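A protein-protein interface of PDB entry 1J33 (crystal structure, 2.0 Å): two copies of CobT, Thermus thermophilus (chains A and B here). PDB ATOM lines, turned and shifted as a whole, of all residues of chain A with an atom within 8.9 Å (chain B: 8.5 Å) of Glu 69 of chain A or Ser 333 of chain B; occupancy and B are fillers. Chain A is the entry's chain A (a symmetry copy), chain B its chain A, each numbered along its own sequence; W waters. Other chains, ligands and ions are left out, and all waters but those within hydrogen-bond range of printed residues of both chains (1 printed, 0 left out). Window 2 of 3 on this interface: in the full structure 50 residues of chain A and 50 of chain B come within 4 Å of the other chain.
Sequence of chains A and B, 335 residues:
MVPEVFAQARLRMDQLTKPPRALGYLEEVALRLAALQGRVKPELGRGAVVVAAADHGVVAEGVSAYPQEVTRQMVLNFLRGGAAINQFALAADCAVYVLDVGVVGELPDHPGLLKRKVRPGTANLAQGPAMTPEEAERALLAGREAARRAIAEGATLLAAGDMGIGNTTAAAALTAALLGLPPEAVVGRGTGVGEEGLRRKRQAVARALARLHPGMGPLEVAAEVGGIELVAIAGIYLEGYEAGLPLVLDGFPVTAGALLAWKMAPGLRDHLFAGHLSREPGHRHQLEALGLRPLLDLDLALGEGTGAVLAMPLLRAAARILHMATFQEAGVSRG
OG of Ser 64 of chain A lies within hydrogen-bond range of N of Tyr 66 of chain A (3.0 Å). O of Phe 327 of chain B sits at hydrogen-bond distance from N of Val 332 of chain B (2.9 Å). OE1 of Glu 69 of chain A is in hydrogen-bond range of NE2 of Gln 73 of chain A (3.1 Å).
The side-chain amide nitrogen (NE2) of Gln 73 of chain A is in hydrogen-bond range of the backbone carbonyl oxygen (O) of Gly 331 of chain B (3.3 Å). OE2 of Glu 69 of chain A lies close to OG of Ser 333 of chain B (3.3 Å). OE1 of Gln 73 of chain A lies within hydrogen-bond range of N of Ser 333 of chain B (3.0 Å).
Ala 65 of chain A touches Gly 335 of chain B (O to CA, 3.97 Å). OH of Tyr 66 of chain A touches O of Lys 18 of chain B, 3.96 Å away. Tyr 66 of chain A touches Arg 334 of chain B (CE1 to O, 3.4 Å). Pro 67 of chain A touches Gly 335 of chain B. CG1 of Val 70 of chain A touches CG1 of Val 332 of chain B, at 3.8 Å. CG2 of Val 70 of chain A touches O of Ser 333 of chain B (3.7 Å). Val 332 of chain B touches Gln 73 of chain A. Thr 17 of chain B touches Met 74 of chain A.
Of the 12 printed residues of chain B, 7 touch a printed residue of chain A. Printed residues of chain B that touch a printed residue of chain A: Thr 17, Lys 18, Gly 331, Val 332, Ser 333, Arg 334 and Gly 335. Among the printed residues, no Asp or Glu carboxylate lies within 4 Å of a Lys or Arg side-chain nitrogen of the other chain.
No position is printed for both chains. Of the 11 pairs that touch across the chains among the printed residues, none has its exchanged pair printed and touching as well.
Of chain B, only Ser 333 comes within 4 Å of Glu 69 of chain A. Ser 333 of chain B touches just these residues of chain A: Glu 69 (3.3 Å), Val 70 (3.7 Å) and Gln 73 (3.0 Å). Printed residues of chain A within 4 Å of Gly 335 of chain B: Ala 65 and Pro 67. Of the printed residues of chain A, Arg 334 of chain B touches Tyr 66. Printed residues of chain B within 4 Å of Pro 67 of chain A: Gly 335 (3.5 Å). Val 59 of chain A touches none of the printed residues of chain B.
Water W1 lies within hydrogen-bond range of O of Ala 330 of chain B (2.7 Å) and O of Gln 73 of chain A (2.9 Å).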
ATOM      1  N   ASP A  55      -4.691  18.349  -2.256  1.00  0.00           N
ATOM      2  CA  ASP A  55      -4.158  17.804  -3.493  1.00  0.00           C
ATOM      3  C   ASP A  55      -2.927  18.583  -3.950  1.00  0.00           C
ATOM      4  O   ASP A  55      -2.695  19.706  -3.504  1.00  0.00           O
ATOM      5  CB  ASP A  55      -5.242  17.816  -4.572  1.00  0.00           C
ATOM      6  CG  ASP A  55      -6.228  16.672  -4.410  1.00  0.00           C
ATOM      7  OD1 ASP A  55      -7.447  16.929  -4.354  1.00  0.00           O
ATOM      8  OD2 ASP A  55      -5.773  15.511  -4.338  1.00  0.00           O
ATOM      9  N   VAL A  59       1.101  16.358  -9.450  1.00  0.00           N
ATOM     10  CA  VAL A  59       0.684  15.048  -9.936  1.00  0.00           C
ATOM     11  C   VAL A  59       0.773  15.054 -11.458  1.00  0.00           C
ATOM     12  O   VAL A  59       0.804  14.002 -12.093  1.00  0.00           O
ATOM     13  CB  VAL A  59      -0.771  14.705  -9.528  1.00  0.00           C
ATOM     14  CG1 VAL A  59      -0.885  14.643  -8.012  1.00  0.00           C
ATOM     15  CG2 VAL A  59      -1.738  15.737 -10.100  1.00  0.00           C
ATOM     16  N   SER A  64       2.836   9.958  -8.879  1.00  0.00           N
ATOM     17  CA  SER A  64       2.066   8.994  -8.096  1.00  0.00           C
ATOM     18  C   SER A  64       1.503   7.861  -8.945  1.00  0.00           C
ATOM     19  O   SER A  64       1.338   8.000 -10.158  1.00  0.00           O
ATOM     20  CB  SER A  64       0.912   9.699  -7.376  1.00  0.00           C
ATOM     21  OG  SER A  64       0.056   8.763  -6.740  1.00  0.00           O
ATOM     22  N   ALA A  65       1.200   6.742  -8.293  1.00  0.00           N
ATOM     23  CA  ALA A  65       0.639   5.580  -8.971  1.00  0.00           C
ATOM     24  C   ALA A  65      -0.881   5.570  -8.821  1.00  0.00           C
ATOM     25  O   ALA A  65      -1.548   4.618  -9.225  1.00  0.00           O
ATOM     26  CB  ALA A  65       1.227   4.301  -8.384  1.00  0.00           C
ATOM     27  N   TYR A  66      -1.421   6.636  -8.238  1.00  0.00           N
ATOM     28  CA  TYR A  66      -2.857   6.752  -8.024  1.00  0.00           C
ATOM     29  C   TYR A  66      -3.432   8.025  -8.641  1.00  0.00           C
ATOM     30  O   TYR A  66      -2.756   9.054  -8.709  1.00  0.00           O
ATOM     31  CB  TYR A  66      -3.155   6.733  -6.522  1.00  0.00           C
ATOM     32  CG  TYR A  66      -3.017   5.370  -5.893  1.00  0.00           C
ATOM     33  CD1 TYR A  66      -3.976   4.383  -6.114  1.00  0.00           C
ATOM     34  CD2 TYR A  66      -1.913   5.052  -5.100  1.00  0.00           C
ATOM     35  CE1 TYR A  66      -3.843   3.111  -5.562  1.00  0.00           C
ATOM     36  CE2 TYR A  66      -1.769   3.780  -4.543  1.00  0.00           C
ATOM     37  CZ  TYR A  66      -2.739   2.816  -4.780  1.00  0.00           C
ATOM     38  OH  TYR A  66      -2.603   1.554  -4.248  1.00  0.00           O
ATOM     39  N   PRO A  67      -4.689   7.969  -9.115  1.00  0.00           N
ATOM     40  CA  PRO A  67      -5.299   9.160  -9.712  1.00  0.00           C
ATOM     41  C   PRO A  67      -5.439  10.221  -8.619  1.00  0.00           C
ATOM     42  O   PRO A  67      -5.506   9.889  -7.439  1.00  0.00           O
ATOM     43  CB  PRO A  67      -6.665   8.657 -10.189  1.00  0.00           C
ATOM     44  CG  PRO A  67      -6.465   7.188 -10.369  1.00  0.00           C
ATOM     45  CD  PRO A  67      -5.601   6.816  -9.200  1.00  0.00           C
ATOM     46  N   GLN A  68      -5.492  11.489  -9.009  1.00  0.00           N
ATOM     47  CA  GLN A  68      -5.629  12.561  -8.038  1.00  0.00           C
ATOM     48  C   GLN A  68      -6.900  12.419  -7.206  1.00  0.00           C
ATOM     49  O   GLN A  68      -6.922  12.771  -6.029  1.00  0.00           O
ATOM     50  CB  GLN A  68      -5.637  13.918  -8.743  1.00  0.00           C
ATOM     51  CG  GLN A  68      -5.773  15.090  -7.791  1.00  0.00           C
ATOM     52  CD  GLN A  68      -5.436  16.409  -8.452  1.00  0.00           C
ATOM     53  OE1 GLN A  68      -6.225  16.949  -9.229  1.00  0.00           O
ATOM     54  NE2 GLN A  68      -4.253  16.932  -8.152  1.00  0.00           N
ATOM     55  N   GLU A  69      -7.951  11.894  -7.827  1.00  0.00           N
ATOM     56  CA  GLU A  69      -9.246  11.720  -7.172  1.00  0.00           C
ATOM     57  C   GLU A  69      -9.226  10.855  -5.910  1.00  0.00           C
ATOM     58  O   GLU A  69     -10.171  10.887  -5.119  1.00  0.00           O
ATOM     59  CB  GLU A  69     -10.246  11.121  -8.164  1.00  0.00           C
ATOM     60  CG  GLU A  69      -9.901   9.707  -8.580  1.00  0.00           C
ATOM     61  CD  GLU A  69     -10.837   9.162  -9.635  1.00  0.00           C
ATOM     62  OE1 GLU A  69     -12.067   9.251  -9.439  1.00  0.00           O
ATOM     63  OE2 GLU A  69     -10.344   8.638 -10.655  1.00  0.00           O
ATOM     64  N   VAL A  70      -8.165  10.073  -5.731  1.00  0.00           N
ATOM     65  CA  VAL A  70      -8.054   9.204  -4.563  1.00  0.00           C
ATOM     66  C   VAL A  70      -8.043   9.992  -3.252  1.00  0.00           C
ATOM     67  O   VAL A  70      -8.527   9.506  -2.227  1.00  0.00           O
ATOM     68  CB  VAL A  70      -6.785   8.323  -4.648  1.00  0.00           C
ATOM     69  CG1 VAL A  70      -6.650   7.470  -3.393  1.00  0.00           C
ATOM     70  CG2 VAL A  70      -6.867   7.420  -5.873  1.00  0.00           C
ATOM     71  N   THR A  71      -7.503  11.207  -3.281  1.00  0.00           N
ATOM     72  CA  THR A  71      -7.460  12.036  -2.076  1.00  0.00           C
ATOM     73  C   THR A  71      -8.879  12.332  -1.592  1.00  0.00           C
ATOM     74  O   THR A  71      -9.225  12.049  -0.445  1.00  0.00           O
ATOM     75  CB  THR A  71      -6.739  13.378  -2.332  1.00  0.00           C
ATOM     76  OG1 THR A  71      -5.420  13.131  -2.832  1.00  0.00           O
ATOM     77  CG2 THR A  71      -6.631  14.164  -1.043  1.00  0.00           C
ATOM     78  N   ARG A  72      -9.705  12.898  -2.467  1.00  0.00           N
ATOM     79  CA  ARG A  72     -11.077  13.210  -2.083  1.00  0.00           C
ATOM     80  C   ARG A  72     -11.804  11.940  -1.655  1.00  0.00           C
ATOM     81  O   ARG A  72     -12.484  11.926  -0.634  1.00  0.00           O
ATOM     82  CB  ARG A  72     -11.837  13.868  -3.244  1.00  0.00           C
ATOM     83  CG  ARG A  72     -13.312  14.119  -2.969  1.00  0.00           C
ATOM     84  CD  ARG A  72     -14.020  14.655  -4.211  1.00  0.00           C
ATOM     85  NE  ARG A  72     -13.862  13.758  -5.354  1.00  0.00           N
ATOM     86  CZ  ARG A  72     -14.333  12.515  -5.404  1.00  0.00           C
ATOM     87  NH1 ARG A  72     -15.000  12.013  -4.374  1.00  0.00           N
ATOM     88  NH2 ARG A  72     -14.127  11.770  -6.482  1.00  0.00           N
ATOM     89  N   GLN A  73     -11.648  10.873  -2.433  1.00  0.00           N
ATOM     90  CA  GLN A  73     -12.307   9.601  -2.128  1.00  0.00           C
ATOM     91  C   GLN A  73     -11.893   9.062  -0.763  1.00  0.00           C
ATOM     92  O   GLN A  73     -12.735   8.579   0.002  1.00  0.00           O
ATOM     93  CB  GLN A  73     -11.999   8.572  -3.220  1.00  0.00           C
ATOM     94  CG  GLN A  73     -12.539   8.964  -4.597  1.00  0.00           C
ATOM     95  CD  GLN A  73     -12.018   8.073  -5.709  1.00  0.00           C
ATOM     96  OE1 GLN A  73     -10.882   7.605  -5.663  1.00  0.00           O
ATOM     97  NE2 GLN A  73     -12.840   7.853  -6.728  1.00  0.00           N
ATOM     98  N   MET A  74     -10.599   9.149  -0.457  1.00  0.00           N
ATOM     99  CA  MET A  74     -10.099   8.679   0.829  1.00  0.00           C
ATOM    100  C   MET A  74     -10.650   9.524   1.972  1.00  0.00           C
ATOM    101  O   MET A  74     -10.896   9.011   3.059  1.00  0.00           O
ATOM    102  CB  MET A  74      -8.566   8.694   0.856  1.00  0.00           C
ATOM    103  CG  MET A  74      -7.942   7.487   0.184  1.00  0.00           C
ATOM    104  SD  MET A  74      -8.512   5.929   0.937  1.00  0.00           S
ATOM    105  CE  MET A  74      -7.585   5.956   2.477  1.00  0.00           C
ATOM    106  N   VAL A  75     -10.843  10.818   1.733  1.00  0.00           N
ATOM    107  CA  VAL A  75     -11.394  11.676   2.776  1.00  0.00           C
ATOM    108  C   VAL A  75     -12.786  11.165   3.154  1.00  0.00           C
ATOM    109  O   VAL A  75     -13.123  11.080   4.342  1.00  0.00           O
ATOM    110  CB  VAL A  75     -11.473  13.150   2.319  1.00  0.00           C
ATOM    111  CG1 VAL A  75     -12.378  13.941   3.249  1.00  0.00           C
ATOM    112  CG2 VAL A  75     -10.074  13.770   2.334  1.00  0.00           C
ATOM    113  N   LEU A  76     -13.589  10.809   2.152  1.00  0.00           N
ATOM    114  CA  LEU A  76     -14.933  10.291   2.418  1.00  0.00           C
ATOM    115  C   LEU A  76     -14.797   8.956   3.162  1.00  0.00           C
ATOM    116  O   LEU A  76     -15.602   8.617   4.031  1.00  0.00           O
ATOM    117  CB  LEU A  76     -15.699  10.099   1.103  1.00  0.00           C
ATOM    118  CG  LEU A  76     -16.005  11.379   0.306  1.00  0.00           C
ATOM    119  CD1 LEU A  76     -16.661  11.029  -1.021  1.00  0.00           C
ATOM    120  CD2 LEU A  76     -16.916  12.286   1.115  1.00  0.00           C
ATOM    121  N   VAL A 103      -8.228  19.942  -0.934  1.00  0.00           N
ATOM    122  CA  VAL A 103      -8.655  18.847  -1.793  1.00  0.00           C
ATOM    123  C   VAL A 103      -9.364  19.422  -3.019  1.00  0.00           C
ATOM    124  O   VAL A 103     -10.092  20.406  -2.919  1.00  0.00           O
ATOM    125  CB  VAL A 103      -9.621  17.887  -1.054  1.00  0.00           C
ATOM    126  CG1 VAL A 103     -10.203  16.878  -2.036  1.00  0.00           C
ATOM    127  CG2 VAL A 103      -8.876  17.151   0.062  1.00  0.00           C
ATOM    128  N   VAL A 104      -9.124  18.817  -4.177  1.00  0.00           N
ATOM    129  CA  VAL A 104      -9.766  19.261  -5.402  1.00  0.00           C
ATOM    130  C   VAL A 104     -11.163  18.667  -5.423  1.00  0.00           C
ATOM    131  O   VAL A 104     -11.330  17.449  -5.501  1.00  0.00           O
ATOM    132  CB  VAL A 104      -9.003  18.780  -6.648  1.00  0.00           C
ATOM    133  CG1 VAL A 104      -9.824  19.064  -7.906  1.00  0.00           C
ATOM    134  CG2 VAL A 104      -7.651  19.476  -6.725  1.00  0.00           C
ATOM    135  N   GLY A 105     -12.168  19.532  -5.343  1.00  0.00           N
ATOM    136  CA  GLY A 105     -13.535  19.060  -5.353  1.00  0.00           C
ATOM    137  C   GLY A 105     -14.268  19.391  -4.072  1.00  0.00           C
ATOM    138  O   GLY A 105     -13.667  19.550  -3.009  1.00  0.00           O
ATOM    139  N   LEU A 107     -16.863  18.908  -0.853  1.00  0.00           N
ATOM    140  CA  LEU A 107     -17.074  17.886   0.160  1.00  0.00           C
ATOM    141  C   LEU A 107     -18.275  18.298   0.995  1.00  0.00           C
ATOM    142  O   LEU A 107     -18.374  19.444   1.431  1.00  0.00           O
ATOM    143  CB  LEU A 107     -15.845  17.758   1.062  1.00  0.00           C
ATOM    144  CG  LEU A 107     -14.595  17.128   0.446  1.00  0.00           C
ATOM    145  CD1 LEU A 107     -13.418  17.336   1.382  1.00  0.00           C
ATOM    146  CD2 LEU A 107     -14.838  15.644   0.191  1.00  0.00           C
ATOM    147  N   MET A 163      -3.027  13.074   3.887  1.00  0.00           N
ATOM    148  CA  MET A 163      -3.737  12.440   2.789  1.00  0.00           C
ATOM    149  C   MET A 163      -3.645  13.426   1.638  1.00  0.00           C
ATOM    150  O   MET A 163      -4.243  14.501   1.676  1.00  0.00           O
ATOM    151  CB  MET A 163      -5.206  12.167   3.130  1.00  0.00           C
ATOM    152  CG  MET A 163      -5.936  11.340   2.056  1.00  0.00           C
ATOM    153  SD  MET A 163      -5.215   9.682   1.747  1.00  0.00           S
ATOM    154  CE  MET A 163      -4.623   9.816   0.045  1.00  0.00           C
ATOM    155  N   GLY A 164      -2.861  13.061   0.634  1.00  0.00           N
ATOM    156  CA  GLY A 164      -2.684  13.911  -0.520  1.00  0.00           C
ATOM    157  C   GLY A 164      -1.859  13.178  -1.553  1.00  0.00           C
ATOM    158  O   GLY A 164      -0.645  12.999  -1.389  1.00  0.00           O
ATOM    159  N   ILE A 165      -2.517  12.723  -2.610  1.00  0.00           N
ATOM    160  CA  ILE A 165      -1.818  12.016  -3.670  1.00  0.00           C
ATOM    161  C   ILE A 165      -0.712  12.925  -4.199  1.00  0.00           C
ATOM    162  O   ILE A 165      -0.953  14.093  -4.540  1.00  0.00           O
ATOM    163  CB  ILE A 165      -2.791  11.631  -4.807  1.00  0.00           C
ATOM    164  CG1 ILE A 165      -3.800  10.598  -4.286  1.00  0.00           C
ATOM    165  CG2 ILE A 165      -2.028  11.060  -5.999  1.00  0.00           C
ATOM    166  CD1 ILE A 165      -3.155   9.314  -3.744  1.00  0.00           C
ATOM    167  N   LEU B  16      -7.618  -3.961   0.177  1.00  0.00           N
ATOM    168  CA  LEU B  16      -7.878  -2.923   1.170  1.00  0.00           C
ATOM    169  C   LEU B  16      -7.460  -1.561   0.619  1.00  0.00           C
ATOM    170  O   LEU B  16      -6.592  -1.486  -0.246  1.00  0.00           O
ATOM    171  CB  LEU B  16      -7.125  -3.236   2.469  1.00  0.00           C
ATOM    172  CG  LEU B  16      -7.560  -4.552   3.127  1.00  0.00           C
ATOM    173  CD1 LEU B  16      -6.881  -4.722   4.488  1.00  0.00           C
ATOM    174  CD2 LEU B  16      -9.078  -4.552   3.292  1.00  0.00           C
ATOM    175  N   THR B  17      -8.084  -0.492   1.116  1.00  0.00           N
ATOM    176  CA  THR B  17      -7.784   0.857   0.649  1.00  0.00           C
ATOM    177  C   THR B  17      -6.454   1.408   1.145  1.00  0.00           C
ATOM    178  O   THR B  17      -6.398   2.191   2.094  1.00  0.00           O
ATOM    179  CB  THR B  17      -8.905   1.859   1.026  1.00  0.00           C
ATOM    180  OG1 THR B  17      -9.140   1.829   2.442  1.00  0.00           O
ATOM    181  CG2 THR B  17     -10.195   1.511   0.288  1.00  0.00           C
ATOM    182  N   LYS B  18      -5.385   0.985   0.482  1.00  0.00           N
ATOM    183  CA  LYS B  18      -4.028   1.427   0.786  1.00  0.00           C
ATOM    184  C   LYS B  18      -3.087   0.799  -0.223  1.00  0.00           C
ATOM    185  O   LYS B  18      -3.405  -0.239  -0.808  1.00  0.00           O
ATOM    186  CB  LYS B  18      -3.622   1.040   2.214  1.00  0.00           C
ATOM    187  CG  LYS B  18      -3.949  -0.380   2.639  1.00  0.00           C
ATOM    188  CD  LYS B  18      -3.032  -1.395   2.026  1.00  0.00           C
ATOM    189  CE  LYS B  18      -3.248  -2.751   2.665  1.00  0.00           C
ATOM    190  NZ  LYS B  18      -2.496  -3.782   1.923  1.00  0.00           N
ATOM    191  N   THR B 326     -12.450  -2.178   1.276  1.00  0.00           N
ATOM    192  CA  THR B 326     -11.687  -2.494   0.080  1.00  0.00           C
ATOM    193  C   THR B 326     -11.961  -1.312  -0.839  1.00  0.00           C
ATOM    194  O   THR B 326     -12.799  -0.465  -0.525  1.00  0.00           O
ATOM    195  CB  THR B 326     -12.190  -3.777  -0.605  1.00  0.00           C
ATOM    196  OG1 THR B 326     -13.568  -3.613  -0.957  1.00  0.00           O
ATOM    197  CG2 THR B 326     -12.050  -4.972   0.328  1.00  0.00           C
ATOM    198  N   PHE B 327     -11.256  -1.249  -1.961  1.00  0.00           N
ATOM    199  CA  PHE B 327     -11.431  -0.160  -2.914  1.00  0.00           C
ATOM    200  C   PHE B 327     -12.873  -0.068  -3.410  1.00  0.00           C
ATOM    201  O   PHE B 327     -13.436   1.023  -3.502  1.00  0.00           O
ATOM    202  CB  PHE B 327     -10.474  -0.349  -4.094  1.00  0.00           C
ATOM    203  CG  PHE B 327      -9.050   0.024  -3.779  1.00  0.00           C
ATOM    204  CD1 PHE B 327      -8.636   1.352  -3.850  1.00  0.00           C
ATOM    205  CD2 PHE B 327      -8.127  -0.946  -3.393  1.00  0.00           C
ATOM    206  CE1 PHE B 327      -7.323   1.711  -3.543  1.00  0.00           C
ATOM    207  CE2 PHE B 327      -6.810  -0.595  -3.083  1.00  0.00           C
ATOM    208  CZ  PHE B 327      -6.409   0.733  -3.160  1.00  0.00           C
ATOM    209  N   GLN B 328     -13.462  -1.217  -3.721  1.00  0.00           N
ATOM    210  CA  GLN B 328     -14.837  -1.268  -4.202  1.00  0.00           C
ATOM    211  C   GLN B 328     -15.810  -0.853  -3.105  1.00  0.00           C
ATOM    212  O   GLN B 328     -16.730  -0.072  -3.348  1.00  0.00           O
ATOM    213  CB  GLN B 328     -15.182  -2.681  -4.687  1.00  0.00           C
ATOM    214  CG  GLN B 328     -14.538  -3.077  -6.016  1.00  0.00           C
ATOM    215  CD  GLN B 328     -14.946  -2.157  -7.161  1.00  0.00           C
ATOM    216  OE1 GLN B 328     -14.394  -1.070  -7.324  1.00  0.00           O
ATOM    217  NE2 GLN B 328     -15.928  -2.586  -7.948  1.00  0.00           N
ATOM    218  N   ALA B 330     -15.307   1.087  -0.686  1.00  0.00           N
ATOM    219  CA  ALA B 330     -15.163   2.507  -0.355  1.00  0.00           C
ATOM    220  C   ALA B 330     -15.318   3.464  -1.536  1.00  0.00           C
ATOM    221  O   ALA B 330     -15.306   4.683  -1.360  1.00  0.00           O
ATOM    222  CB  ALA B 330     -13.802   2.746   0.325  1.00  0.00           C
ATOM    223  N   GLY B 331     -15.456   2.925  -2.738  1.00  0.00           N
ATOM    224  CA  GLY B 331     -15.599   3.781  -3.901  1.00  0.00           C
ATOM    225  C   GLY B 331     -14.319   4.535  -4.208  1.00  0.00           C
ATOM    226  O   GLY B 331     -14.355   5.659  -4.719  1.00  0.00           O
ATOM    227  N   VAL B 332     -13.184   3.921  -3.887  1.00  0.00           N
ATOM    228  CA  VAL B 332     -11.880   4.525  -4.135  1.00  0.00           C
ATOM    229  C   VAL B 332     -11.236   3.875  -5.355  1.00  0.00           C
ATOM    230  O   VAL B 332     -11.156   2.648  -5.446  1.00  0.00           O
ATOM    231  CB  VAL B 332     -10.932   4.342  -2.924  1.00  0.00           C
ATOM    232  CG1 VAL B 332      -9.590   5.003  -3.204  1.00  0.00           C
ATOM    233  CG2 VAL B 332     -11.563   4.937  -1.665  1.00  0.00           C
ATOM    234  N   SER B 333     -10.787   4.698  -6.298  1.00  0.00           N
ATOM    235  CA  SER B 333     -10.136   4.192  -7.504  1.00  0.00           C
ATOM    236  C   SER B 333      -8.818   3.528  -7.108  1.00  0.00           C
ATOM    237  O   SER B 333      -8.144   3.980  -6.183  1.00  0.00           O
ATOM    238  CB  SER B 333      -9.864   5.340  -8.478  1.00  0.00           C
ATOM    239  OG  SER B 333     -11.064   6.022  -8.803  1.00  0.00           O
ATOM    240  N   ARG B 334      -8.450   2.460  -7.808  1.00  0.00           N
ATOM    241  CA  ARG B 334      -7.216   1.750  -7.488  1.00  0.00           C
ATOM    242  C   ARG B 334      -6.061   2.096  -8.420  1.00  0.00           C
ATOM    243  O   ARG B 334      -4.995   1.482  -8.349  1.00  0.00           O
ATOM    244  CB  ARG B 334      -7.454   0.238  -7.512  1.00  0.00           C
ATOM    245  CG  ARG B 334      -6.863  -0.474  -6.309  1.00  0.00           C
ATOM    246  CD  ARG B 334      -7.032  -1.978  -6.391  1.00  0.00           C
ATOM    247  NE  ARG B 334      -6.068  -2.575  -7.308  1.00  0.00           N
ATOM    248  CZ  ARG B 334      -6.042  -3.864  -7.629  1.00  0.00           C
ATOM    249  NH1 ARG B 334      -6.933  -4.697  -7.109  1.00  0.00           N
ATOM    250  NH2 ARG B 334      -5.119  -4.319  -8.466  1.00  0.00           N
ATOM    251  N   GLY B 335      -6.269   3.082  -9.284  1.00  0.00           N
ATOM    252  CA  GLY B 335      -5.222   3.476 -10.207  1.00  0.00           C
ATOM    253  C   GLY B 335      -5.738   3.695 -11.616  1.00  0.00           C
ATOM    254  O   GLY B 335      -6.958   3.537 -11.838  1.00  0.00           O
ATOM    255  OXT GLY B 335      -4.919   4.029 -12.501  1.00  0.00           O
HETATM  256  O   HOH W   1     -15.138   7.315  -0.981  1.00  0.00           O
